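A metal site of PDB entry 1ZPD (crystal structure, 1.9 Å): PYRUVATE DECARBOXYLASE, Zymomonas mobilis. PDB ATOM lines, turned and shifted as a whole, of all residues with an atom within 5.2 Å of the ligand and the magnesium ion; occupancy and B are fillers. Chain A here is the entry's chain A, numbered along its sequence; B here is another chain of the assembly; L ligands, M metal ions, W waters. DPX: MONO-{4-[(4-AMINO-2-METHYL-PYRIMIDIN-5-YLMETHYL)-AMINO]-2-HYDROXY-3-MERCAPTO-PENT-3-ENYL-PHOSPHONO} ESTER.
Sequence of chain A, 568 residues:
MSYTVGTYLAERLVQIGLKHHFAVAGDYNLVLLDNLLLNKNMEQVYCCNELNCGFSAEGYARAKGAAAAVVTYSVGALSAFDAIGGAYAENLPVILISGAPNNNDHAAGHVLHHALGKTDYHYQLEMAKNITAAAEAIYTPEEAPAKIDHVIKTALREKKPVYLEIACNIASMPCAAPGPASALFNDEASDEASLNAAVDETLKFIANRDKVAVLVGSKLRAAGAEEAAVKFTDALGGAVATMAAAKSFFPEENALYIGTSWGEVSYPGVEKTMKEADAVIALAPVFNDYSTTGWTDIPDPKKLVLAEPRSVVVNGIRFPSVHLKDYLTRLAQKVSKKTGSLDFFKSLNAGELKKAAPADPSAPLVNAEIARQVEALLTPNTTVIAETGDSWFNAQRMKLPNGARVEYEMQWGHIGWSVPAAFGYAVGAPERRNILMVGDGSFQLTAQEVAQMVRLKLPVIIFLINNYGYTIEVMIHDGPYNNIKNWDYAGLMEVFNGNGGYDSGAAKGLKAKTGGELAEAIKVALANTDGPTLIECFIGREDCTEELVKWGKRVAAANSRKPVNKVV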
ATOM      1  N   GLU A 387     -21.222 -16.127  25.762  1.00  0.00           N
ATOM      2  CA  GLU A 387     -21.099 -14.655  25.809  1.00  0.00           C
ATOM      3  C   GLU A 387     -20.585 -14.179  27.153  1.00  0.00           C
ATOM      4  O   GLU A 387     -20.875 -14.744  28.218  1.00  0.00           O
ATOM      5  CB  GLU A 387     -22.485 -14.033  25.568  1.00  0.00           C
ATOM      6  CG  GLU A 387     -22.525 -12.489  25.501  1.00  0.00           C
ATOM      7  CD  GLU A 387     -21.668 -11.919  24.379  1.00  0.00           C
ATOM      8  OE1 GLU A 387     -20.442 -11.793  24.581  1.00  0.00           O
ATOM      9  OE2 GLU A 387     -22.202 -11.617  23.293  1.00  0.00           O
ATOM     10  N   THR A 388     -19.876 -13.041  27.103  1.00  0.00           N
ATOM     11  CA  THR A 388     -19.560 -12.275  28.304  1.00  0.00           C
ATOM     12  C   THR A 388     -20.836 -12.018  29.121  1.00  0.00           C
ATOM     13  O   THR A 388     -21.836 -11.467  28.625  1.00  0.00           O
ATOM     14  CB  THR A 388     -18.882 -10.923  27.957  1.00  0.00           C
ATOM     15  OG1 THR A 388     -17.631 -11.204  27.281  1.00  0.00           O
ATOM     16  CG2 THR A 388     -18.600 -10.117  29.219  1.00  0.00           C
ATOM     17  N   GLY A 389     -20.767 -12.375  30.379  1.00  0.00           N
ATOM     18  CA  GLY A 389     -21.911 -12.259  31.301  1.00  0.00           C
ATOM     19  C   GLY A 389     -21.921 -13.516  32.187  1.00  0.00           C
ATOM     20  O   GLY A 389     -20.908 -14.230  32.216  1.00  0.00           O
ATOM     21  N   ASP A 390     -23.048 -13.822  32.852  1.00  0.00           N
ATOM     22  CA  ASP A 390     -23.064 -15.050  33.683  1.00  0.00           C
ATOM     23  C   ASP A 390     -22.937 -16.319  32.850  1.00  0.00           C
ATOM     24  O   ASP A 390     -22.504 -17.365  33.370  1.00  0.00           O
ATOM     25  CB  ASP A 390     -24.277 -15.107  34.613  1.00  0.00           C
ATOM     26  CG  ASP A 390     -24.027 -16.005  35.820  1.00  0.00           C
ATOM     27  OD1 ASP A 390     -22.879 -16.152  36.320  1.00  0.00           O
ATOM     28  OD2 ASP A 390     -25.028 -16.587  36.312  1.00  0.00           O
ATOM     29  N   SER A 391     -23.209 -16.268  31.560  1.00  0.00           N
ATOM     30  CA  SER A 391     -22.961 -17.381  30.640  1.00  0.00           C
ATOM     31  C   SER A 391     -21.480 -17.801  30.641  1.00  0.00           C
ATOM     32  O   SER A 391     -21.230 -18.978  30.331  1.00  0.00           O
ATOM     33  CB  SER A 391     -23.389 -17.042  29.212  1.00  0.00           C
ATOM     34  OG  SER A 391     -24.792 -16.914  29.072  1.00  0.00           O
ATOM     35  N   GLY A 413     -13.777  -9.263  25.394  1.00  0.00           N
ATOM     36  CA  GLY A 413     -14.994  -9.155  26.190  1.00  0.00           C
ATOM     37  C   GLY A 413     -15.974  -8.073  25.732  1.00  0.00           C
ATOM     38  O   GLY A 413     -16.519  -7.339  26.567  1.00  0.00           O
ATOM     39  N   HIS A 414     -16.236  -7.982  24.439  1.00  0.00           N
ATOM     40  CA  HIS A 414     -17.214  -7.048  23.894  1.00  0.00           C
ATOM     41  C   HIS A 414     -18.611  -7.682  23.938  1.00  0.00           C
ATOM     42  O   HIS A 414     -18.855  -8.608  23.141  1.00  0.00           O
ATOM     43  CB  HIS A 414     -16.839  -6.694  22.458  1.00  0.00           C
ATOM     44  CG  HIS A 414     -17.714  -5.711  21.738  1.00  0.00           C
ATOM     45  ND1 HIS A 414     -19.076  -5.893  21.570  1.00  0.00           N
ATOM     46  CD2 HIS A 414     -17.411  -4.517  21.147  1.00  0.00           C
ATOM     47  CE1 HIS A 414     -19.574  -4.851  20.903  1.00  0.00           C
ATOM     48  NE2 HIS A 414     -18.592  -3.994  20.644  1.00  0.00           N
ATOM     49  N   ILE A 415     -19.477  -7.233  24.859  1.00  0.00           N
ATOM     50  CA  ILE A 415     -20.809  -7.865  24.948  1.00  0.00           C
ATOM     51  C   ILE A 415     -21.500  -7.679  23.602  1.00  0.00           C
ATOM     52  O   ILE A 415     -21.348  -6.667  22.894  1.00  0.00           O
ATOM     53  CB  ILE A 415     -21.702  -7.374  26.102  1.00  0.00           C
ATOM     54  CG1 ILE A 415     -21.935  -5.843  26.002  1.00  0.00           C
ATOM     55  CG2 ILE A 415     -21.110  -7.753  27.455  1.00  0.00           C
ATOM     56  CD1 ILE A 415     -23.128  -5.413  26.871  1.00  0.00           C
ATOM     57  N   GLY A 439     -26.762 -13.517  27.054  1.00  0.00           N
ATOM     58  CA  GLY A 439     -27.654 -12.777  27.935  1.00  0.00           C
ATOM     59  C   GLY A 439     -28.472 -11.729  27.189  1.00  0.00           C
ATOM     60  O   GLY A 439     -28.115 -11.330  26.079  1.00  0.00           O
ATOM     61  N   ASP A 440     -29.560 -11.246  27.802  1.00  0.00           N
ATOM     62  CA  ASP A 440     -30.434 -10.240  27.188  1.00  0.00           C
ATOM     63  C   ASP A 440     -29.701  -8.927  26.889  1.00  0.00           C
ATOM     64  O   ASP A 440     -29.876  -8.374  25.799  1.00  0.00           O
ATOM     65  CB  ASP A 440     -31.651  -9.958  28.095  1.00  0.00           C
ATOM     66  CG  ASP A 440     -31.339  -9.596  29.522  1.00  0.00           C
ATOM     67  OD1 ASP A 440     -30.292  -9.930  30.112  1.00  0.00           O
ATOM     68  OD2 ASP A 440     -32.206  -8.924  30.145  1.00  0.00           O
ATOM     69  N   GLY A 441     -28.895  -8.448  27.838  1.00  0.00           N
ATOM     70  CA  GLY A 441     -28.184  -7.169  27.618  1.00  0.00           C
ATOM     71  C   GLY A 441     -27.249  -7.226  26.421  1.00  0.00           C
ATOM     72  O   GLY A 441     -27.252  -6.319  25.568  1.00  0.00           O
ATOM     73  N   SER A 442     -26.434  -8.296  26.347  1.00  0.00           N
ATOM     74  CA  SER A 442     -25.521  -8.478  25.223  1.00  0.00           C
ATOM     75  C   SER A 442     -26.265  -8.621  23.908  1.00  0.00           C
ATOM     76  O   SER A 442     -25.840  -8.056  22.891  1.00  0.00           O
ATOM     77  CB  SER A 442     -24.656  -9.748  25.426  1.00  0.00           C
ATOM     78  OG  SER A 442     -23.893  -9.674  26.615  1.00  0.00           O
ATOM     79  N   PHE A 443     -27.365  -9.393  23.908  1.00  0.00           N
ATOM     80  CA  PHE A 443     -28.118  -9.655  22.696  1.00  0.00           C
ATOM     81  C   PHE A 443     -28.533  -8.372  21.980  1.00  0.00           C
ATOM     82  O   PHE A 443     -28.486  -8.266  20.760  1.00  0.00           O
ATOM     83  CB  PHE A 443     -29.366 -10.510  23.014  1.00  0.00           C
ATOM     84  CG  PHE A 443     -30.126 -11.029  21.819  1.00  0.00           C
ATOM     85  CD1 PHE A 443     -29.639 -12.094  21.076  1.00  0.00           C
ATOM     86  CD2 PHE A 443     -31.352 -10.481  21.468  1.00  0.00           C
ATOM     87  CE1 PHE A 443     -30.348 -12.570  19.986  1.00  0.00           C
ATOM     88  CE2 PHE A 443     -32.071 -10.938  20.382  1.00  0.00           C
ATOM     89  CZ  PHE A 443     -31.564 -12.002  19.637  1.00  0.00           C
ATOM     90  N   LEU A 445     -27.037  -5.571  21.595  1.00  0.00           N
ATOM     91  CA  LEU A 445     -26.045  -4.790  20.832  1.00  0.00           C
ATOM     92  C   LEU A 445     -25.957  -5.191  19.377  1.00  0.00           C
ATOM     93  O   LEU A 445     -25.591  -4.403  18.486  1.00  0.00           O
ATOM     94  CB  LEU A 445     -24.644  -4.889  21.457  1.00  0.00           C
ATOM     95  CG  LEU A 445     -24.387  -4.004  22.674  1.00  0.00           C
ATOM     96  CD1 LEU A 445     -24.815  -4.727  23.960  1.00  0.00           C
ATOM     97  CD2 LEU A 445     -22.914  -3.617  22.763  1.00  0.00           C
ATOM     98  N   ILE A 465     -30.817 -15.622  27.831  1.00  0.00           N
ATOM     99  CA  ILE A 465     -31.013 -15.624  29.279  1.00  0.00           C
ATOM    100  C   ILE A 465     -31.666 -14.288  29.687  1.00  0.00           C
ATOM    101  O   ILE A 465     -30.962 -13.264  29.771  1.00  0.00           O
ATOM    102  CB  ILE A 465     -29.708 -15.898  30.036  1.00  0.00           C
ATOM    103  CG1 ILE A 465     -28.935 -17.091  29.436  1.00  0.00           C
ATOM    104  CG2 ILE A 465     -29.958 -16.139  31.519  1.00  0.00           C
ATOM    105  CD1 ILE A 465     -29.705 -18.411  29.369  1.00  0.00           C
ATOM    106  N   ASN A 467     -32.818 -12.245  32.278  1.00  0.00           N
ATOM    107  CA  ASN A 467     -32.841 -11.845  33.675  1.00  0.00           C
ATOM    108  C   ASN A 467     -33.072 -10.322  33.797  1.00  0.00           C
ATOM    109  O   ASN A 467     -32.780  -9.743  34.846  1.00  0.00           O
ATOM    110  CB  ASN A 467     -31.551 -12.281  34.375  1.00  0.00           C
ATOM    111  CG  ASN A 467     -30.263 -11.796  33.725  1.00  0.00           C
ATOM    112  OD1 ASN A 467     -30.289 -10.925  32.848  1.00  0.00           O
ATOM    113  ND2 ASN A 467     -29.120 -12.315  34.151  1.00  0.00           N
ATOM    114  N   TYR A 468     -33.565  -9.682  32.754  1.00  0.00           N
ATOM    115  CA  TYR A 468     -33.944  -8.255  32.794  1.00  0.00           C
ATOM    116  C   TYR A 468     -32.792  -7.356  33.228  1.00  0.00           C
ATOM    117  O   TYR A 468     -32.928  -6.643  34.231  1.00  0.00           O
ATOM    118  CB  TYR A 468     -35.207  -8.053  33.641  1.00  0.00           C
ATOM    119  CG  TYR A 468     -35.954  -6.741  33.423  1.00  0.00           C
ATOM    120  CD1 TYR A 468     -36.054  -6.122  32.183  1.00  0.00           C
ATOM    121  CD2 TYR A 468     -36.564  -6.108  34.502  1.00  0.00           C
ATOM    122  CE1 TYR A 468     -36.734  -4.920  32.011  1.00  0.00           C
ATOM    123  CE2 TYR A 468     -37.262  -4.900  34.353  1.00  0.00           C
ATOM    124  CZ  TYR A 468     -37.342  -4.320  33.105  1.00  0.00           C
ATOM    125  OH  TYR A 468     -38.022  -3.120  32.942  1.00  0.00           O
ATOM    126  N   GLY A 469     -31.694  -7.335  32.456  1.00  0.00           N
ATOM    127  CA  GLY A 469     -30.631  -6.334  32.713  1.00  0.00           C
ATOM    128  C   GLY A 469     -29.228  -6.948  32.729  1.00  0.00           C
ATOM    129  O   GLY A 469     -29.012  -8.118  32.383  1.00  0.00           O
ATOM    130  N   TYR A 470     -28.258  -6.180  33.231  1.00  0.00           N
ATOM    131  CA  TYR A 470     -26.840  -6.575  33.212  1.00  0.00           C
ATOM    132  C   TYR A 470     -26.409  -7.192  34.540  1.00  0.00           C
ATOM    133  O   TYR A 470     -25.798  -6.507  35.370  1.00  0.00           O
ATOM    134  CB  TYR A 470     -25.957  -5.352  32.893  1.00  0.00           C
ATOM    135  CG  TYR A 470     -26.142  -4.556  31.631  1.00  0.00           C
ATOM    136  CD1 TYR A 470     -26.579  -5.109  30.439  1.00  0.00           C
ATOM    137  CD2 TYR A 470     -25.842  -3.187  31.622  1.00  0.00           C
ATOM    138  CE1 TYR A 470     -26.712  -4.353  29.287  1.00  0.00           C
ATOM    139  CE2 TYR A 470     -25.984  -2.402  30.476  1.00  0.00           C
ATOM    140  CZ  TYR A 470     -26.419  -2.989  29.308  1.00  0.00           C
ATOM    141  OH  TYR A 470     -26.550  -2.207  28.181  1.00  0.00           O
ATOM    142  N   THR A 471     -26.667  -8.497  34.770  1.00  0.00           N
ATOM    143  CA  THR A 471     -26.428  -9.071  36.096  1.00  0.00           C
ATOM    144  C   THR A 471     -24.953  -9.066  36.465  1.00  0.00           C
ATOM    145  O   THR A 471     -24.618  -8.769  37.614  1.00  0.00           O
ATOM    146  CB  THR A 471     -27.049 -10.493  36.200  1.00  0.00           C
ATOM    147  OG1 THR A 471     -28.477 -10.332  36.405  1.00  0.00           O
ATOM    148  CG2 THR A 471     -26.502 -11.307  37.371  1.00  0.00           C
ATOM    149  N   ILE A 472     -24.049  -9.403  35.540  1.00  0.00           N
ATOM    150  CA  ILE A 472     -22.618  -9.382  35.876  1.00  0.00           C
ATOM    151  C   ILE A 472     -22.202  -7.981  36.319  1.00  0.00           C
ATOM    152  O   ILE A 472     -21.491  -7.862  37.307  1.00  0.00           O
ATOM    153  CB  ILE A 472     -21.715  -9.863  34.722  1.00  0.00           C
ATOM    154  CG1 ILE A 472     -20.237  -9.814  35.130  1.00  0.00           C
ATOM    155  CG2 ILE A 472     -21.920  -9.036  33.457  1.00  0.00           C
ATOM    156  CD1 ILE A 472     -19.509  -8.557  34.680  1.00  0.00           C
ATOM    157  N   GLU A 473     -22.678  -6.903  35.676  1.00  0.00           N
ATOM    158  CA  GLU A 473     -22.404  -5.540  36.117  1.00  0.00           C
ATOM    159  C   GLU A 473     -23.055  -5.205  37.455  1.00  0.00           C
ATOM    160  O   GLU A 473     -22.428  -4.611  38.339  1.00  0.00           O
ATOM    161  CB  GLU A 473     -22.833  -4.538  35.028  1.00  0.00           C
ATOM    162  CG  GLU A 473     -21.873  -3.388  34.780  1.00  0.00           C
ATOM    163  CD  GLU A 473     -20.620  -3.786  34.013  1.00  0.00           C
ATOM    164  OE1 GLU A 473     -19.911  -4.749  34.386  1.00  0.00           O
ATOM    165  OE2 GLU A 473     -20.326  -3.098  32.999  1.00  0.00           O
ATOM    166  N   VAL B  24     -23.421   4.147  27.821  1.00  0.00           N
ATOM    167  CA  VAL B  24     -23.542   2.662  27.905  1.00  0.00           C
ATOM    168  C   VAL B  24     -22.563   2.222  29.003  1.00  0.00           C
ATOM    169  O   VAL B  24     -21.346   2.477  28.933  1.00  0.00           O
ATOM    170  CB  VAL B  24     -23.192   1.904  26.627  1.00  0.00           C
ATOM    171  CG1 VAL B  24     -23.323   0.377  26.898  1.00  0.00           C
ATOM    172  CG2 VAL B  24     -24.048   2.306  25.448  1.00  0.00           C
ATOM    173  N   ALA B  25     -23.074   1.580  30.057  1.00  0.00           N
ATOM    174  CA  ALA B  25     -22.283   1.166  31.190  1.00  0.00           C
ATOM    175  C   ALA B  25     -21.186   0.144  30.820  1.00  0.00           C
ATOM    176  O   ALA B  25     -21.322  -0.673  29.908  1.00  0.00           O
ATOM    177  CB  ALA B  25     -23.174   0.524  32.262  1.00  0.00           C
ATOM    178  N   GLY B  26     -20.116   0.219  31.570  1.00  0.00           N
ATOM    179  CA  GLY B  26     -19.004  -0.752  31.554  1.00  0.00           C
ATOM    180  C   GLY B  26     -18.204  -0.560  32.821  1.00  0.00           C
ATOM    181  O   GLY B  26     -18.193   0.581  33.322  1.00  0.00           O
ATOM    182  N   ASP B  27     -17.473  -1.583  33.304  1.00  0.00           N
ATOM    183  CA  ASP B  27     -16.820  -1.456  34.605  1.00  0.00           C
ATOM    184  C   ASP B  27     -15.799  -0.308  34.657  1.00  0.00           C
ATOM    185  O   ASP B  27     -15.614   0.255  35.745  1.00  0.00           O
ATOM    186  CB  ASP B  27     -16.203  -2.784  35.038  1.00  0.00           C
ATOM    187  CG  ASP B  27     -15.109  -3.398  34.178  1.00  0.00           C
ATOM    188  OD1 ASP B  27     -14.919  -2.986  33.005  1.00  0.00           O
ATOM    189  OD2 ASP B  27     -14.444  -4.318  34.716  1.00  0.00           O
ATOM    190  N   GLU B  50     -22.700   1.228  21.595  1.00  0.00           N
ATOM    191  CA  GLU B  50     -21.935   2.476  21.609  1.00  0.00           C
ATOM    192  C   GLU B  50     -21.943   3.220  20.290  1.00  0.00           C
ATOM    193  O   GLU B  50     -21.784   4.469  20.274  1.00  0.00           O
ATOM    194  CB  GLU B  50     -20.503   2.192  22.128  1.00  0.00           C
ATOM    195  CG  GLU B  50     -20.462   1.789  23.594  1.00  0.00           C
ATOM    196  CD  GLU B  50     -20.614   0.284  23.861  1.00  0.00           C
ATOM    197  OE1 GLU B  50     -20.866  -0.452  22.893  1.00  0.00           O
ATOM    198  OE2 GLU B  50     -20.452  -0.140  25.026  1.00  0.00           O
ATOM    199  N   THR B  72     -17.328   2.754  27.631  1.00  0.00           N
ATOM    200  CA  THR B  72     -16.266   2.055  28.340  1.00  0.00           C
ATOM    201  C   THR B  72     -15.005   1.938  27.477  1.00  0.00           C
ATOM    202  O   THR B  72     -15.080   2.047  26.249  1.00  0.00           O
ATOM    203  CB  THR B  72     -16.710   0.684  28.904  1.00  0.00           C
ATOM    204  OG1 THR B  72     -15.772   0.272  29.900  1.00  0.00           O
ATOM    205  CG2 THR B  72     -16.782  -0.386  27.810  1.00  0.00           C
ATOM    206  N   VAL B  75     -13.517  -1.486  23.921  1.00  0.00           N
ATOM    207  CA  VAL B  75     -14.698  -2.103  23.324  1.00  0.00           C
ATOM    208  C   VAL B  75     -15.856  -1.105  23.186  1.00  0.00           C
ATOM    209  O   VAL B  75     -16.632  -1.294  22.254  1.00  0.00           O
ATOM    210  CB  VAL B  75     -15.161  -3.360  24.114  1.00  0.00           C
ATOM    211  CG1 VAL B  75     -14.070  -4.450  24.080  1.00  0.00           C
ATOM    212  CG2 VAL B  75     -15.531  -3.045  25.552  1.00  0.00           C
ATOM    213  N   GLY B  76     -15.986  -0.098  24.066  1.00  0.00           N
ATOM    214  CA  GLY B  76     -17.032   0.903  23.845  1.00  0.00           C
ATOM    215  C   GLY B  76     -16.567   2.083  22.970  1.00  0.00           C
ATOM    216  O   GLY B  76     -17.266   2.530  22.058  1.00  0.00           O
ATOM    217  N   HIS B 114     -10.425  -5.918  27.900  1.00  0.00           N
ATOM    218  CA  HIS B 114     -10.909  -5.007  26.872  1.00  0.00           C
ATOM    219  C   HIS B 114      -9.796  -4.401  25.996  1.00  0.00           C
ATOM    220  O   HIS B 114     -10.155  -3.757  24.981  1.00  0.00           O
ATOM    221  CB  HIS B 114     -11.780  -3.861  27.393  1.00  0.00           C
ATOM    222  CG  HIS B 114     -13.089  -4.213  28.038  1.00  0.00           C
ATOM    223  ND1 HIS B 114     -13.768  -5.392  27.793  1.00  0.00           N
ATOM    224  CD2 HIS B 114     -13.861  -3.503  28.912  1.00  0.00           C
ATOM    225  CE1 HIS B 114     -14.880  -5.414  28.515  1.00  0.00           C
ATOM    226  NE2 HIS B 114     -14.981  -4.282  29.199  1.00  0.00           N
HETATM  227  C4  DPX L   1     -21.651  -5.252  30.358  1.00  0.00           C
HETATM  228  C5  DPX L   1     -22.082  -6.505  30.768  1.00  0.00           C
HETATM  229  O21 DPX L   1     -27.462  -9.331  30.017  1.00  0.00           O
HETATM  230  O22 DPX L   1     -25.553 -10.781  30.980  1.00  0.00           O
HETATM  231  O26 DPX L   1     -24.655 -10.448  33.138  1.00  0.00           O
HETATM  232  O25 DPX L   1     -25.534 -12.629  32.710  1.00  0.00           O
HETATM  233  O24 DPX L   1     -27.083 -10.655  32.759  1.00  0.00           O
HETATM  234  P23 DPX L   1     -25.732 -11.215  32.463  1.00  0.00           P
HETATM  235  P19 DPX L   1     -26.054  -9.717  29.888  1.00  0.00           P
HETATM  236  O20 DPX L   1     -25.657  -9.965  28.530  1.00  0.00           O
HETATM  237  O18 DPX L   1     -25.328  -8.296  30.323  1.00  0.00           O
HETATM  238  C17 DPX L   1     -23.897  -8.183  30.176  1.00  0.00           C
HETATM  239  C16 DPX L   1     -23.506  -7.007  31.052  1.00  0.00           C
HETATM  240  C15 DPX L   1     -22.592  -4.092  30.093  1.00  0.00           C
HETATM  241  N3  DPX L   1     -20.324  -5.111  30.175  1.00  0.00           N
HETATM  242  S1  DPX L   1     -20.789  -7.649  31.041  1.00  0.00           S
HETATM  243  C6  DPX L   1     -19.676  -3.772  29.727  1.00  0.00           C
HETATM  244  C7  DPX L   1     -19.557  -3.619  28.232  1.00  0.00           C
HETATM  245  C8  DPX L   1     -18.766  -4.564  27.427  1.00  0.00           C
HETATM  246  N9  DPX L   1     -18.682  -4.407  26.089  1.00  0.00           N
HETATM  247  C10 DPX L   1     -19.322  -3.417  25.499  1.00  0.00           C
HETATM  248  N11 DPX L   1     -19.912  -2.398  26.214  1.00  0.00           N
HETATM  249  C12 DPX L   1     -20.138  -2.592  27.540  1.00  0.00           C
HETATM  250  N13 DPX L   1     -18.144  -5.596  28.032  1.00  0.00           N
HETATM  251  C14 DPX L   1     -19.260  -3.240  24.044  1.00  0.00           C
HETATM  252 MG    MG M   1     -28.918 -10.102  31.462  1.00  0.00          MG
HETATM  253  O   HOH W   1     -24.415 -12.335  28.199  1.00  0.00           O
HETATM  254  O   HOH W   2     -25.046 -14.399  30.041  1.00  0.00           O
HETATM  255  O   HOH W   3     -17.460  -6.514  30.752  1.00  0.00           O
HETATM  256  O   HOH W   4     -28.673 -12.225  30.929  1.00  0.00           O
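The side-chain hydroxyl (OG) of Ser 442 lies within hydrogen-bond range of the backbone carbonyl oxygen (O) of Thr 388, at 3.4 Å. The side-chain carboxylate (OE2) of Glu 473 lies within hydrogen-bond range of the backbone NH (N) of Asp 27 of chain B (3.2 Å). OD2 of Asp 440 sits at hydrogen-bond distance from N of Tyr 468 (3.0 Å). The backbone carbonyl oxygen (O) of Ile 465 is in hydrogen-bond range of the backbone NH (N) of Asp 440, 3.1 Å away. ND2 of Asn 467 lies within hydrogen-bond range of OG1 of Thr 471.
O21 of the ligand lies close to N of Gly 441 (2.8 Å). The backbone carbonyl oxygen (O) of Gly 413 sits at hydrogen-bond distance from a nitrogen (N13) of the ligand, at 2.8 Å. The backbone NH (N) of Ile 415 sits at hydrogen-bond distance from a nitrogen (N9) of the ligand (3.2 Å). The side-chain hydroxyl (OG) of Ser 442 is in hydrogen-bond range of an oxygen (O20) of the ligand (2.6 Å). O25 of the ligand lies within hydrogen-bond range of N of Asp 390, at 2.8 Å. The backbone NH (N) of Ile 472 is in hydrogen-bond range of an oxygen (O26) of the ligand, 2.7 Å away. N11 of the ligand is in hydrogen-bond range of OE2 of Glu 50 of chain B. The backbone NH (N) of Thr 471 sits at hydrogen-bond distance from an oxygen (O26) of the ligand (3.2 Å). O20 of the ligand sits at hydrogen-bond distance from N of Ser 442, at 2.9 Å. OE2 of Glu 473 lies close to N3 of the ligand, at 3.5 Å.
N of Gly 441 touches the magnesium ion (3.98 Å). Within 4 Å of the magnesium ion: Asp 440, Gly 441, Asn 467 and Gly 469.
The magnesium ion is bound by OD1 of Asp 440 (1.9 Å), OD1 of Asn 467 (2.1 Å), O of Gly 469 (2.2 Å), O21 of the ligand (2.2 Å), water W4 (2.2 Å) and O24 of the ligand (2.3 Å). The magnesium ion has six donor atoms within binding distance.
Water W4 lies within hydrogen-bond range of O of Ile 465 (2.8 Å), ND2 of Asn 467 (3.3 Å), N of Asp 440 (3.4 Å) and O22 of the ligand (3.4 Å). Water W1 lies within hydrogen-bond range of O20 of the ligand (2.7 Å), O of Thr 388 (2.8 Å), N of Gly 439 (2.9 Å) and OG of Ser 442 (3.1 Å). Water W2 lies within hydrogen-bond range of OG of Ser 391, O25 of the ligand and N of Asp 390.
Residues that only touch the ligand: Ala 25 of chain B, His 114 of chain B, Tyr 470, Val 75 of chain B, Gly 439, His 414, Gly 26 of chain B, Gly 389, Thr 388 and Leu 445. Hydrophobic or aromatic side chains that line the ligand: His 414, Ile 415, Leu 445, Tyr 470, Ile 472, Val 75 of chain B and His 114 of chain B. Within 4 Å of the ligand: Thr 388, Gly 389, Asp 390, Gly 413, His 414, Ile 415, Gly 439, Asp 440, Gly 441, Ser 442, Leu 445, Asn 467, Gly 469, Tyr 470, Thr 471, Ile 472, Glu 473, Ala 25 of chain B, Gly 26 of chain B, Glu 50 of chain B, Val 75 of chain B and His 114 of chain B. The nearest printed residue that does not touch the ligand is Thr 72 of chain B (4.03 Å).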
